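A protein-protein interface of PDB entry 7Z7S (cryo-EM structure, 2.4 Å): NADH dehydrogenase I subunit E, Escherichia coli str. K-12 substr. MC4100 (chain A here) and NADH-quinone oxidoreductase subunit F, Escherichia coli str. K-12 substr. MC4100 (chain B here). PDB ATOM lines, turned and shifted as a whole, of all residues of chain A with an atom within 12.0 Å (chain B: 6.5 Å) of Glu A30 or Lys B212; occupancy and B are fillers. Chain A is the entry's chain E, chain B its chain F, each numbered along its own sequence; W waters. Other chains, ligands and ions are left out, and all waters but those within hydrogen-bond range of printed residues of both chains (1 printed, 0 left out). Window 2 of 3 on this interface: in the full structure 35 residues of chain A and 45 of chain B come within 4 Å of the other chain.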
ATOM      1  N   ILE A  22      11.865 -31.337 -24.642  1.00  0.00           N
ATOM      2  CA  ILE A  22      12.448 -29.998 -24.652  1.00  0.00           C
ATOM      3  C   ILE A  22      11.437 -28.962 -24.170  1.00  0.00           C
ATOM      4  O   ILE A  22      11.781 -28.065 -23.394  1.00  0.00           O
ATOM      5  CB  ILE A  22      12.994 -29.668 -26.055  1.00  0.00           C
ATOM      6  CG1 ILE A  22      14.238 -30.502 -26.341  1.00  0.00           C
ATOM      7  CG2 ILE A  22      13.367 -28.208 -26.162  1.00  0.00           C
ATOM      8  CD1 ILE A  22      14.722 -30.409 -27.761  1.00  0.00           C
ATOM      9  N   GLU A  23      10.173 -29.076 -24.589  1.00  0.00           N
ATOM     10  CA  GLU A  23       9.165 -28.120 -24.125  1.00  0.00           C
ATOM     11  C   GLU A  23       8.860 -28.292 -22.638  1.00  0.00           C
ATOM     12  O   GLU A  23       8.657 -27.301 -21.918  1.00  0.00           O
ATOM     13  CB  GLU A  23       7.888 -28.245 -24.953  1.00  0.00           C
ATOM     14  CG  GLU A  23       8.089 -28.010 -26.433  1.00  0.00           C
ATOM     15  CD  GLU A  23       7.636 -26.639 -26.880  1.00  0.00           C
ATOM     16  OE1 GLU A  23       7.265 -25.818 -26.016  1.00  0.00           O
ATOM     17  OE2 GLU A  23       7.659 -26.377 -28.101  1.00  0.00           O
ATOM     18  N   HIS A  24       8.839 -29.539 -22.157  1.00  0.00           N
ATOM     19  CA  HIS A  24       8.638 -29.775 -20.732  1.00  0.00           C
ATOM     20  C   HIS A  24       9.777 -29.188 -19.914  1.00  0.00           C
ATOM     21  O   HIS A  24       9.560 -28.680 -18.809  1.00  0.00           O
ATOM     22  CB  HIS A  24       8.499 -31.269 -20.454  1.00  0.00           C
ATOM     23  CG  HIS A  24       8.241 -31.588 -19.015  1.00  0.00           C
ATOM     24  ND1 HIS A  24       7.311 -30.908 -18.258  1.00  0.00           N
ATOM     25  CD2 HIS A  24       8.799 -32.505 -18.191  1.00  0.00           C
ATOM     26  CE1 HIS A  24       7.302 -31.398 -17.031  1.00  0.00           C
ATOM     27  NE2 HIS A  24       8.196 -32.367 -16.964  1.00  0.00           N
ATOM     28  N   GLU A  25      11.000 -29.244 -20.436  1.00  0.00           N
ATOM     29  CA  GLU A  25      12.094 -28.584 -19.739  1.00  0.00           C
ATOM     30  C   GLU A  25      12.040 -27.071 -19.886  1.00  0.00           C
ATOM     31  O   GLU A  25      12.551 -26.352 -19.023  1.00  0.00           O
ATOM     32  CB  GLU A  25      13.425 -29.125 -20.233  1.00  0.00           C
ATOM     33  CG  GLU A  25      13.776 -30.412 -19.551  1.00  0.00           C
ATOM     34  CD  GLU A  25      14.387 -30.184 -18.186  1.00  0.00           C
ATOM     35  OE1 GLU A  25      15.306 -29.345 -18.080  1.00  0.00           O
ATOM     36  OE2 GLU A  25      13.951 -30.843 -17.221  1.00  0.00           O
ATOM     37  N   MET A  26      11.435 -26.577 -20.966  1.00  0.00           N
ATOM     38  CA  MET A  26      11.220 -25.144 -21.115  1.00  0.00           C
ATOM     39  C   MET A  26      10.260 -24.615 -20.062  1.00  0.00           C
ATOM     40  O   MET A  26      10.351 -23.444 -19.680  1.00  0.00           O
ATOM     41  CB  MET A  26      10.679 -24.833 -22.507  1.00  0.00           C
ATOM     42  CG  MET A  26      11.726 -24.502 -23.531  1.00  0.00           C
ATOM     43  SD  MET A  26      11.122 -24.810 -25.195  1.00  0.00           S
ATOM     44  CE  MET A  26      10.244 -23.285 -25.507  1.00  0.00           C
ATOM     45  N   HIS A  27       9.333 -25.452 -19.588  1.00  0.00           N
ATOM     46  CA  HIS A  27       8.417 -25.016 -18.534  1.00  0.00           C
ATOM     47  C   HIS A  27       9.109 -24.757 -17.197  1.00  0.00           C
ATOM     48  O   HIS A  27       8.540 -24.065 -16.350  1.00  0.00           O
ATOM     49  CB  HIS A  27       7.312 -26.051 -18.323  1.00  0.00           C
ATOM     50  CG  HIS A  27       6.414 -26.225 -19.503  1.00  0.00           C
ATOM     51  ND1 HIS A  27       5.827 -27.431 -19.819  1.00  0.00           N
ATOM     52  CD2 HIS A  27       6.006 -25.348 -20.450  1.00  0.00           C
ATOM     53  CE1 HIS A  27       5.094 -27.289 -20.908  1.00  0.00           C
ATOM     54  NE2 HIS A  27       5.184 -26.034 -21.310  1.00  0.00           N
ATOM     55  N   HIS A  28      10.312 -25.288 -16.985  1.00  0.00           N
ATOM     56  CA  HIS A  28      10.946 -25.255 -15.673  1.00  0.00           C
ATOM     57  C   HIS A  28      11.613 -23.927 -15.346  1.00  0.00           C
ATOM     58  O   HIS A  28      12.019 -23.728 -14.198  1.00  0.00           O
ATOM     59  CB  HIS A  28      11.991 -26.366 -15.571  1.00  0.00           C
ATOM     60  CG  HIS A  28      11.408 -27.742 -15.539  1.00  0.00           C
ATOM     61  ND1 HIS A  28      10.052 -27.978 -15.588  1.00  0.00           N
ATOM     62  CD2 HIS A  28      12.000 -28.957 -15.479  1.00  0.00           C
ATOM     63  CE1 HIS A  28       9.833 -29.280 -15.553  1.00  0.00           C
ATOM     64  NE2 HIS A  28      10.999 -29.896 -15.486  1.00  0.00           N
ATOM     65  N   TYR A  29      11.746 -23.024 -16.307  1.00  0.00           N
ATOM     66  CA  TYR A  29      12.470 -21.780 -16.111  1.00  0.00           C
ATOM     67  C   TYR A  29      11.607 -20.617 -16.567  1.00  0.00           C
ATOM     68  O   TYR A  29      10.554 -20.795 -17.179  1.00  0.00           O
ATOM     69  CB  TYR A  29      13.797 -21.781 -16.879  1.00  0.00           C
ATOM     70  CG  TYR A  29      14.599 -23.048 -16.722  1.00  0.00           C
ATOM     71  CD1 TYR A  29      15.445 -23.223 -15.639  1.00  0.00           C
ATOM     72  CD2 TYR A  29      14.518 -24.063 -17.662  1.00  0.00           C
ATOM     73  CE1 TYR A  29      16.179 -24.374 -15.492  1.00  0.00           C
ATOM     74  CE2 TYR A  29      15.248 -25.218 -17.521  1.00  0.00           C
ATOM     75  CZ  TYR A  29      16.079 -25.367 -16.437  1.00  0.00           C
ATOM     76  OH  TYR A  29      16.813 -26.517 -16.291  1.00  0.00           O
ATOM     77  N   GLU A  30      12.064 -19.411 -16.256  1.00  0.00           N
ATOM     78  CA  GLU A  30      11.415 -18.198 -16.727  1.00  0.00           C
ATOM     79  C   GLU A  30      11.959 -17.724 -18.066  1.00  0.00           C
ATOM     80  O   GLU A  30      11.445 -16.749 -18.620  1.00  0.00           O
ATOM     81  CB  GLU A  30      11.556 -17.092 -15.681  1.00  0.00           C
ATOM     82  CG  GLU A  30      12.981 -16.709 -15.376  1.00  0.00           C
ATOM     83  CD  GLU A  30      13.093 -15.309 -14.832  1.00  0.00           C
ATOM     84  OE1 GLU A  30      12.993 -15.142 -13.600  1.00  0.00           O
ATOM     85  OE2 GLU A  30      13.282 -14.374 -15.634  1.00  0.00           O
ATOM     86  N   ASP A  31      12.978 -18.394 -18.603  1.00  0.00           N
ATOM     87  CA  ASP A  31      13.532 -18.103 -19.910  1.00  0.00           C
ATOM     88  C   ASP A  31      13.714 -19.434 -20.629  1.00  0.00           C
ATOM     89  O   ASP A  31      14.304 -20.364 -20.057  1.00  0.00           O
ATOM     90  CB  ASP A  31      14.866 -17.365 -19.810  1.00  0.00           C
ATOM     91  CG  ASP A  31      15.131 -16.470 -20.997  1.00  0.00           C
ATOM     92  OD1 ASP A  31      15.173 -16.975 -22.134  1.00  0.00           O
ATOM     93  OD2 ASP A  31      15.317 -15.258 -20.794  1.00  0.00           O
ATOM     94  N   PRO A  32      13.219 -19.567 -21.863  1.00  0.00           N
ATOM     95  CA  PRO A  32      13.440 -20.817 -22.611  1.00  0.00           C
ATOM     96  C   PRO A  32      14.894 -21.073 -22.967  1.00  0.00           C
ATOM     97  O   PRO A  32      15.236 -22.221 -23.268  1.00  0.00           O
ATOM     98  CB  PRO A  32      12.586 -20.640 -23.871  1.00  0.00           C
ATOM     99  CG  PRO A  32      12.243 -19.213 -23.936  1.00  0.00           C
ATOM    100  CD  PRO A  32      12.366 -18.614 -22.586  1.00  0.00           C
ATOM    101  N   ARG A  33      15.751 -20.047 -22.949  1.00  0.00           N
ATOM    102  CA  ARG A  33      17.174 -20.240 -23.215  1.00  0.00           C
ATOM    103  C   ARG A  33      17.818 -21.156 -22.185  1.00  0.00           C
ATOM    104  O   ARG A  33      18.764 -21.881 -22.500  1.00  0.00           O
ATOM    105  CB  ARG A  33      17.880 -18.883 -23.245  1.00  0.00           C
ATOM    106  CG  ARG A  33      19.374 -18.932 -23.501  1.00  0.00           C
ATOM    107  CD  ARG A  33      20.034 -17.618 -23.140  1.00  0.00           C
ATOM    108  NE  ARG A  33      19.673 -16.576 -24.090  1.00  0.00           N
ATOM    109  CZ  ARG A  33      20.253 -16.409 -25.268  1.00  0.00           C
ATOM    110  NH1 ARG A  33      21.258 -17.173 -25.657  1.00  0.00           N
ATOM    111  NH2 ARG A  33      19.810 -15.455 -26.077  1.00  0.00           N
ATOM    112  N   ALA A  34      17.279 -21.179 -20.967  1.00  0.00           N
ATOM    113  CA  ALA A  34      17.794 -22.006 -19.886  1.00  0.00           C
ATOM    114  C   ALA A  34      17.610 -23.497 -20.124  1.00  0.00           C
ATOM    115  O   ALA A  34      18.180 -24.296 -19.378  1.00  0.00           O
ATOM    116  CB  ALA A  34      17.129 -21.599 -18.579  1.00  0.00           C
ATOM    117  N   ALA A  35      16.836 -23.892 -21.132  1.00  0.00           N
ATOM    118  CA  ALA A  35      16.661 -25.289 -21.492  1.00  0.00           C
ATOM    119  C   ALA A  35      17.609 -25.744 -22.595  1.00  0.00           C
ATOM    120  O   ALA A  35      17.428 -26.837 -23.129  1.00  0.00           O
ATOM    121  CB  ALA A  35      15.216 -25.545 -21.916  1.00  0.00           C
ATOM    122  N   SER A  36      18.613 -24.936 -22.947  1.00  0.00           N
ATOM    123  CA  SER A  36      19.481 -25.274 -24.074  1.00  0.00           C
ATOM    124  C   SER A  36      20.397 -26.447 -23.754  1.00  0.00           C
ATOM    125  O   SER A  36      20.579 -27.344 -24.590  1.00  0.00           O
ATOM    126  CB  SER A  36      20.298 -24.052 -24.491  1.00  0.00           C
ATOM    127  OG  SER A  36      21.300 -23.754 -23.540  1.00  0.00           O
ATOM    128  N   LEU A  62      13.769 -23.347 -29.153  1.00  0.00           N
ATOM    129  CA  LEU A  62      13.941 -22.450 -28.016  1.00  0.00           C
ATOM    130  C   LEU A  62      13.849 -20.975 -28.380  1.00  0.00           C
ATOM    131  O   LEU A  62      13.815 -20.140 -27.473  1.00  0.00           O
ATOM    132  CB  LEU A  62      15.284 -22.697 -27.341  1.00  0.00           C
ATOM    133  CG  LEU A  62      15.594 -24.110 -26.873  1.00  0.00           C
ATOM    134  CD1 LEU A  62      17.025 -24.145 -26.466  1.00  0.00           C
ATOM    135  CD2 LEU A  62      14.715 -24.504 -25.726  1.00  0.00           C
ATOM    136  N   GLY A  63      13.835 -20.627 -29.662  1.00  0.00           N
ATOM    137  CA  GLY A  63      13.752 -19.231 -30.033  1.00  0.00           C
ATOM    138  C   GLY A  63      15.007 -18.431 -29.786  1.00  0.00           C
ATOM    139  O   GLY A  63      14.937 -17.207 -29.681  1.00  0.00           O
ATOM    140  N   ILE A  64      16.156 -19.088 -29.681  1.00  0.00           N
ATOM    141  CA  ILE A  64      17.437 -18.412 -29.493  1.00  0.00           C
ATOM    142  C   ILE A  64      18.260 -18.667 -30.752  1.00  0.00           C
ATOM    143  O   ILE A  64      17.931 -19.585 -31.511  1.00  0.00           O
ATOM    144  CB  ILE A  64      18.140 -18.894 -28.210  1.00  0.00           C
ATOM    145  CG1 ILE A  64      18.578 -20.352 -28.332  1.00  0.00           C
ATOM    146  CG2 ILE A  64      17.231 -18.713 -27.013  1.00  0.00           C
ATOM    147  CD1 ILE A  64      19.251 -20.881 -27.094  1.00  0.00           C
ATOM    148  N   MET B  82      10.684  -6.678  -5.412  1.00  0.00           N
ATOM    149  CA  MET B  82      11.387  -7.844  -5.945  1.00  0.00           C
ATOM    150  C   MET B  82      10.898  -9.080  -5.198  1.00  0.00           C
ATOM    151  O   MET B  82      11.485  -9.530  -4.212  1.00  0.00           O
ATOM    152  CB  MET B  82      12.893  -7.668  -5.820  1.00  0.00           C
ATOM    153  CG  MET B  82      13.396  -6.326  -6.303  1.00  0.00           C
ATOM    154  SD  MET B  82      15.115  -6.034  -5.862  1.00  0.00           S
ATOM    155  CE  MET B  82      15.474  -4.588  -6.847  1.00  0.00           C
ATOM    156  N   ILE B  84      10.384 -12.053  -6.804  1.00  0.00           N
ATOM    157  CA  ILE B  84      10.846 -13.243  -7.507  1.00  0.00           C
ATOM    158  C   ILE B  84      12.273 -13.520  -7.062  1.00  0.00           C
ATOM    159  O   ILE B  84      13.168 -12.697  -7.282  1.00  0.00           O
ATOM    160  CB  ILE B  84      10.760 -13.058  -9.029  1.00  0.00           C
ATOM    161  CG1 ILE B  84       9.300 -13.023  -9.482  1.00  0.00           C
ATOM    162  CG2 ILE B  84      11.514 -14.153  -9.749  1.00  0.00           C
ATOM    163  CD1 ILE B  84       8.459 -14.154  -8.933  1.00  0.00           C
ATOM    164  N   ARG B  85      12.492 -14.670  -6.428  1.00  0.00           N
ATOM    165  CA  ARG B  85      13.788 -14.957  -5.838  1.00  0.00           C
ATOM    166  C   ARG B  85      14.171 -16.419  -6.030  1.00  0.00           C
ATOM    167  O   ARG B  85      13.319 -17.328  -6.062  1.00  0.00           O
ATOM    168  CB  ARG B  85      13.811 -14.596  -4.352  1.00  0.00           C
ATOM    169  CG  ARG B  85      14.249 -13.185  -4.071  1.00  0.00           C
ATOM    170  CD  ARG B  85      13.638 -12.672  -2.794  1.00  0.00           C
ATOM    171  NE  ARG B  85      13.447 -11.230  -2.815  1.00  0.00           N
ATOM    172  CZ  ARG B  85      13.981 -10.391  -1.940  1.00  0.00           C
ATOM    173  NH1 ARG B  85      14.750 -10.819  -0.955  1.00  0.00           N
ATOM    174  NH2 ARG B  85      13.734  -9.091  -2.055  1.00  0.00           N
ATOM    175  N   TYR B  86      15.484 -16.629  -6.132  1.00  0.00           N
ATOM    176  CA  TYR B  86      16.032 -17.927  -6.482  1.00  0.00           C
ATOM    177  C   TYR B  86      17.054 -18.393  -5.461  1.00  0.00           C
ATOM    178  O   TYR B  86      17.902 -17.620  -5.002  1.00  0.00           O
ATOM    179  CB  TYR B  86      16.662 -17.890  -7.864  1.00  0.00           C
ATOM    180  CG  TYR B  86      15.650 -17.678  -8.949  1.00  0.00           C
ATOM    181  CD1 TYR B  86      14.790 -18.696  -9.321  1.00  0.00           C
ATOM    182  CD2 TYR B  86      15.544 -16.459  -9.596  1.00  0.00           C
ATOM    183  CE1 TYR B  86      13.861 -18.507 -10.307  1.00  0.00           C
ATOM    184  CE2 TYR B  86      14.613 -16.262 -10.583  1.00  0.00           C
ATOM    185  CZ  TYR B  86      13.774 -17.291 -10.933  1.00  0.00           C
ATOM    186  OH  TYR B  86      12.843 -17.104 -11.920  1.00  0.00           O
ATOM    187  N   TYR B 126      11.020 -18.076  -4.150  1.00  0.00           N
ATOM    188  CA  TYR B 126       9.940 -18.865  -4.711  1.00  0.00           C
ATOM    189  C   TYR B 126      10.446 -20.054  -5.506  1.00  0.00           C
ATOM    190  O   TYR B 126       9.696 -21.017  -5.687  1.00  0.00           O
ATOM    191  CB  TYR B 126       9.041 -17.978  -5.573  1.00  0.00           C
ATOM    192  CG  TYR B 126       9.321 -18.036  -7.055  1.00  0.00           C
ATOM    193  CD1 TYR B 126      10.462 -17.454  -7.587  1.00  0.00           C
ATOM    194  CD2 TYR B 126       8.430 -18.642  -7.925  1.00  0.00           C
ATOM    195  CE1 TYR B 126      10.718 -17.502  -8.931  1.00  0.00           C
ATOM    196  CE2 TYR B 126       8.678 -18.685  -9.275  1.00  0.00           C
ATOM    197  CZ  TYR B 126       9.821 -18.108  -9.771  1.00  0.00           C
ATOM    198  OH  TYR B 126      10.081 -18.147 -11.119  1.00  0.00           O
ATOM    199  N   ARG B 127      11.691 -20.030  -5.990  1.00  0.00           N
ATOM    200  CA  ARG B 127      12.155 -21.190  -6.739  1.00  0.00           C
ATOM    201  C   ARG B 127      13.538 -21.626  -6.287  1.00  0.00           C
ATOM    202  O   ARG B 127      14.364 -20.811  -5.867  1.00  0.00           O
ATOM    203  CB  ARG B 127      12.159 -20.918  -8.238  1.00  0.00           C
ATOM    204  CG  ARG B 127      11.276 -21.854  -9.032  1.00  0.00           C
ATOM    205  CD  ARG B 127      11.035 -21.315 -10.427  1.00  0.00           C
ATOM    206  NE  ARG B 127       9.811 -21.834 -11.020  1.00  0.00           N
ATOM    207  CZ  ARG B 127       9.447 -21.631 -12.277  1.00  0.00           C
ATOM    208  NH1 ARG B 127      10.182 -20.906 -13.100  1.00  0.00           N
ATOM    209  NH2 ARG B 127       8.315 -22.169 -12.720  1.00  0.00           N
ATOM    210  N   TYR B 129      16.824 -24.384  -7.442  1.00  0.00           N
ATOM    211  CA  TYR B 129      17.435 -25.273  -8.420  1.00  0.00           C
ATOM    212  C   TYR B 129      18.650 -25.934  -7.801  1.00  0.00           C
ATOM    213  O   TYR B 129      19.469 -25.260  -7.175  1.00  0.00           O
ATOM    214  CB  TYR B 129      17.849 -24.520  -9.685  1.00  0.00           C
ATOM    215  CG  TYR B 129      16.703 -23.933 -10.467  1.00  0.00           C
ATOM    216  CD1 TYR B 129      16.033 -24.683 -11.417  1.00  0.00           C
ATOM    217  CD2 TYR B 129      16.297 -22.627 -10.257  1.00  0.00           C
ATOM    218  CE1 TYR B 129      14.988 -24.148 -12.130  1.00  0.00           C
ATOM    219  CE2 TYR B 129      15.258 -22.088 -10.964  1.00  0.00           C
ATOM    220  CZ  TYR B 129      14.607 -22.850 -11.899  1.00  0.00           C
ATOM    221  OH  TYR B 129      13.567 -22.310 -12.607  1.00  0.00           O
ATOM    222  N   PRO B 204      25.392 -11.887  -6.690  1.00  0.00           N
ATOM    223  CA  PRO B 204      24.119 -12.535  -7.044  1.00  0.00           C
ATOM    224  C   PRO B 204      22.975 -12.227  -6.099  1.00  0.00           C
ATOM    225  O   PRO B 204      21.817 -12.402  -6.491  1.00  0.00           O
ATOM    226  CB  PRO B 204      24.468 -14.025  -7.010  1.00  0.00           C
ATOM    227  CG  PRO B 204      25.893 -14.070  -7.315  1.00  0.00           C
ATOM    228  CD  PRO B 204      26.502 -12.857  -6.701  1.00  0.00           C
ATOM    229  N   ALA B 205      23.265 -11.772  -4.878  1.00  0.00           N
ATOM    230  CA  ALA B 205      22.220 -11.435  -3.919  1.00  0.00           C
ATOM    231  C   ALA B 205      21.321 -10.313  -4.416  1.00  0.00           C
ATOM    232  O   ALA B 205      20.137 -10.286  -4.077  1.00  0.00           O
ATOM    233  CB  ALA B 205      22.847 -11.053  -2.580  1.00  0.00           C
ATOM    234  N   THR B 206      21.845  -9.392  -5.219  1.00  0.00           N
ATOM    235  CA  THR B 206      21.032  -8.296  -5.734  1.00  0.00           C
ATOM    236  C   THR B 206      20.583  -8.503  -7.175  1.00  0.00           C
ATOM    237  O   THR B 206      19.435  -8.195  -7.505  1.00  0.00           O
ATOM    238  CB  THR B 206      21.787  -6.969  -5.616  1.00  0.00           C
ATOM    239  OG1 THR B 206      22.987  -7.020  -6.393  1.00  0.00           O
ATOM    240  CG2 THR B 206      22.141  -6.691  -4.167  1.00  0.00           C
ATOM    241  N   SER B 207      21.448  -9.011  -8.051  1.00  0.00           N
ATOM    242  CA  SER B 207      21.032  -9.331  -9.415  1.00  0.00           C
ATOM    243  C   SER B 207      21.802 -10.571  -9.856  1.00  0.00           C
ATOM    244  O   SER B 207      22.945 -10.468 -10.308  1.00  0.00           O
ATOM    245  CB  SER B 207      21.260  -8.162 -10.363  1.00  0.00           C
ATOM    246  OG  SER B 207      22.588  -7.693 -10.295  1.00  0.00           O
ATOM    247  N   GLY B 208      21.167 -11.731  -9.726  1.00  0.00           N
ATOM    248  CA  GLY B 208      21.799 -12.984 -10.073  1.00  0.00           C
ATOM    249  C   GLY B 208      21.148 -13.687 -11.239  1.00  0.00           C
ATOM    250  O   GLY B 208      21.291 -13.260 -12.386  1.00  0.00           O
ATOM    251  N   ALA B 209      20.429 -14.766 -10.954  1.00  0.00           N
ATOM    252  CA  ALA B 209      19.814 -15.574 -11.997  1.00  0.00           C
ATOM    253  C   ALA B 209      18.660 -14.820 -12.636  1.00  0.00           C
ATOM    254  O   ALA B 209      17.684 -14.483 -11.960  1.00  0.00           O
ATOM    255  CB  ALA B 209      19.338 -16.902 -11.418  1.00  0.00           C
ATOM    256  N   TRP B 210      18.788 -14.554 -13.939  1.00  0.00           N
ATOM    257  CA  TRP B 210      17.828 -13.778 -14.728  1.00  0.00           C
ATOM    258  C   TRP B 210      17.595 -12.392 -14.139  1.00  0.00           C
ATOM    259  O   TRP B 210      16.492 -11.853 -14.215  1.00  0.00           O
ATOM    260  CB  TRP B 210      16.501 -14.526 -14.897  1.00  0.00           C
ATOM    261  CG  TRP B 210      16.661 -15.883 -15.497  1.00  0.00           C
ATOM    262  CD1 TRP B 210      16.873 -16.177 -16.806  1.00  0.00           C
ATOM    263  CD2 TRP B 210      16.631 -17.134 -14.806  1.00  0.00           C
ATOM    264  NE1 TRP B 210      16.975 -17.529 -16.979  1.00  0.00           N
ATOM    265  CE2 TRP B 210      16.828 -18.142 -15.764  1.00  0.00           C
ATOM    266  CE3 TRP B 210      16.452 -17.501 -13.472  1.00  0.00           C
ATOM    267  CZ2 TRP B 210      16.855 -19.490 -15.432  1.00  0.00           C
ATOM    268  CZ3 TRP B 210      16.480 -18.837 -13.144  1.00  0.00           C
ATOM    269  CH2 TRP B 210      16.680 -19.816 -14.119  1.00  0.00           C
ATOM    270  N   GLY B 211      18.632 -11.812 -13.537  1.00  0.00           N
ATOM    271  CA  GLY B 211      18.555 -10.498 -12.945  1.00  0.00           C
ATOM    272  C   GLY B 211      17.902 -10.437 -11.585  1.00  0.00           C
ATOM    273  O   GLY B 211      17.919  -9.372 -10.959  1.00  0.00           O
ATOM    274  N   LYS B 212      17.335 -11.525 -11.107  1.00  0.00           N
ATOM    275  CA  LYS B 212      16.624 -11.567  -9.843  1.00  0.00           C
ATOM    276  C   LYS B 212      17.589 -11.791  -8.695  1.00  0.00           C
ATOM    277  O   LYS B 212      18.720 -12.232  -8.901  1.00  0.00           O
ATOM    278  CB  LYS B 212      15.578 -12.675  -9.869  1.00  0.00           C
ATOM    279  CG  LYS B 212      14.647 -12.606 -11.049  1.00  0.00           C
ATOM    280  CD  LYS B 212      13.868 -11.316 -11.047  1.00  0.00           C
ATOM    281  CE  LYS B 212      13.346 -10.991 -12.427  1.00  0.00           C
ATOM    282  NZ  LYS B 212      12.672 -12.152 -13.059  1.00  0.00           N
ATOM    283  N   PRO B 213      17.187 -11.444  -7.474  1.00  0.00           N
ATOM    284  CA  PRO B 213      17.974 -11.840  -6.302  1.00  0.00           C
ATOM    285  C   PRO B 213      18.109 -13.354  -6.193  1.00  0.00           C
ATOM    286  O   PRO B 213      17.131 -14.106  -6.292  1.00  0.00           O
ATOM    287  CB  PRO B 213      17.192 -11.244  -5.126  1.00  0.00           C
ATOM    288  CG  PRO B 213      16.067 -10.467  -5.717  1.00  0.00           C
ATOM    289  CD  PRO B 213      16.271 -10.337  -7.168  1.00  0.00           C
ATOM    290  N   THR B 214      19.345 -13.788  -5.987  1.00  0.00           N
ATOM    291  CA  THR B 214      19.733 -15.184  -6.059  1.00  0.00           C
ATOM    292  C   THR B 214      20.733 -15.463  -4.953  1.00  0.00           C
ATOM    293  O   THR B 214      21.590 -14.630  -4.659  1.00  0.00           O
ATOM    294  CB  THR B 214      20.360 -15.517  -7.423  1.00  0.00           C
ATOM    295  OG1 THR B 214      19.544 -14.989  -8.471  1.00  0.00           O
ATOM    296  CG2 THR B 214      20.482 -16.997  -7.609  1.00  0.00           C
HETATM  297  O   HOH W   1      13.193 -19.540 -13.601  1.00  0.00           O
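O of His A28 lies within hydrogen-bond range of OH of Tyr B129, at 2.6 Å.
The side-chain carboxylate (OE1) of Glu A30 lies within salt-bridge range of the side-chain amino group (NZ) of Lys B212 (3.1 Å).
OE1 of Glu A30 sits at hydrogen-bond distance from OH of Tyr B86 (2.6 Å).
O of Lys B212 sits at hydrogen-bond distance from OG1 of Thr B214 (2.9 Å).
O of His A24 sits close to ND1 of His A28 (3.3 Å).
N of Arg B127 sits at hydrogen-bond distance from O of Arg B85, 3.2 Å away.
The side-chain hydroxyl (OH) of Tyr B126 sits close to the guanidinium group (NH1) of Arg B127.
OH of Tyr B86 is in hydrogen-bond range of OH of Tyr B126, at 3.1 Å.
The side-chain carboxylate (OD1) of Asp A31 sits close to the backbone NH (N) of Arg A33 (3.2 Å).
NH1 of Arg B127 touches O of His A28, 3.5 Å away.
C of Tyr A29 touches NH1 of Arg B127 (3.8 Å).
Tyr B129 touches Tyr A29 (CE1 to CE1, 3.6 Å).
CH2 of Trp B210 touches CD1 of Tyr A29, at 3.9 Å.
Glu A30 touches Arg B127 (N to NH1, 3.97 Å).
Trp B210 touches Glu A30 (CB to OE2, 3.3 Å).
Asp A31 touches Trp B210.
Trp B210 touches Ala A34.
Of the printed residues of chain B, Tyr A29 touches Arg B127 (3.8 Å), Tyr B129 (3.6 Å) and Trp B210 (3.9 Å).
Glu A30 touches just these residues of chain B: Tyr B86, Arg B127, Trp B210 and Lys B212.
Of the printed residues of chain B, Asp A31 touches Trp B210 (3.5 Å).
No residue of chain A comes within 4 Å of Ile B84.
Tyr B86 touches just one residue of chain A: Glu A30.
Of the printed residues of chain A, Arg B127 touches His A28 (3.5 Å), Tyr A29 (3.8 Å) and Glu A30 (3.97 Å).
No residue of chain A comes within 4 Å of Ser B207.
Of chain A, only Tyr A29 (3.9 Å), Glu A30 (3.3 Å), Asp A31 (3.5 Å) and Ala A34 (3.8 Å) come within 4 Å of Trp B210.
Of chain A, only Glu A30 comes within 4 Å of Lys B212.
Thr B214 touches none of the printed residues of chain A.
Of the 18 printed residues of chain B, 5 touch a printed residue of chain A.
Hydrophobic or aromatic side chains of chain B within 4 Å of the printed part of chain A: Tyr B86, Tyr B129 and Trp B210.
Along chain B the printed residues that touch a printed residue of chain A span positions 86 to 212.
Among the printed residues, 11 pairs touch across the chains.
Water W1 lies within hydrogen-bond range of N of Glu A30 (2.9 Å), OH of Tyr B129 (3.0 Å), OH of Tyr B86 (3.0 Å) and NH1 of Arg B127 (3.3 Å).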
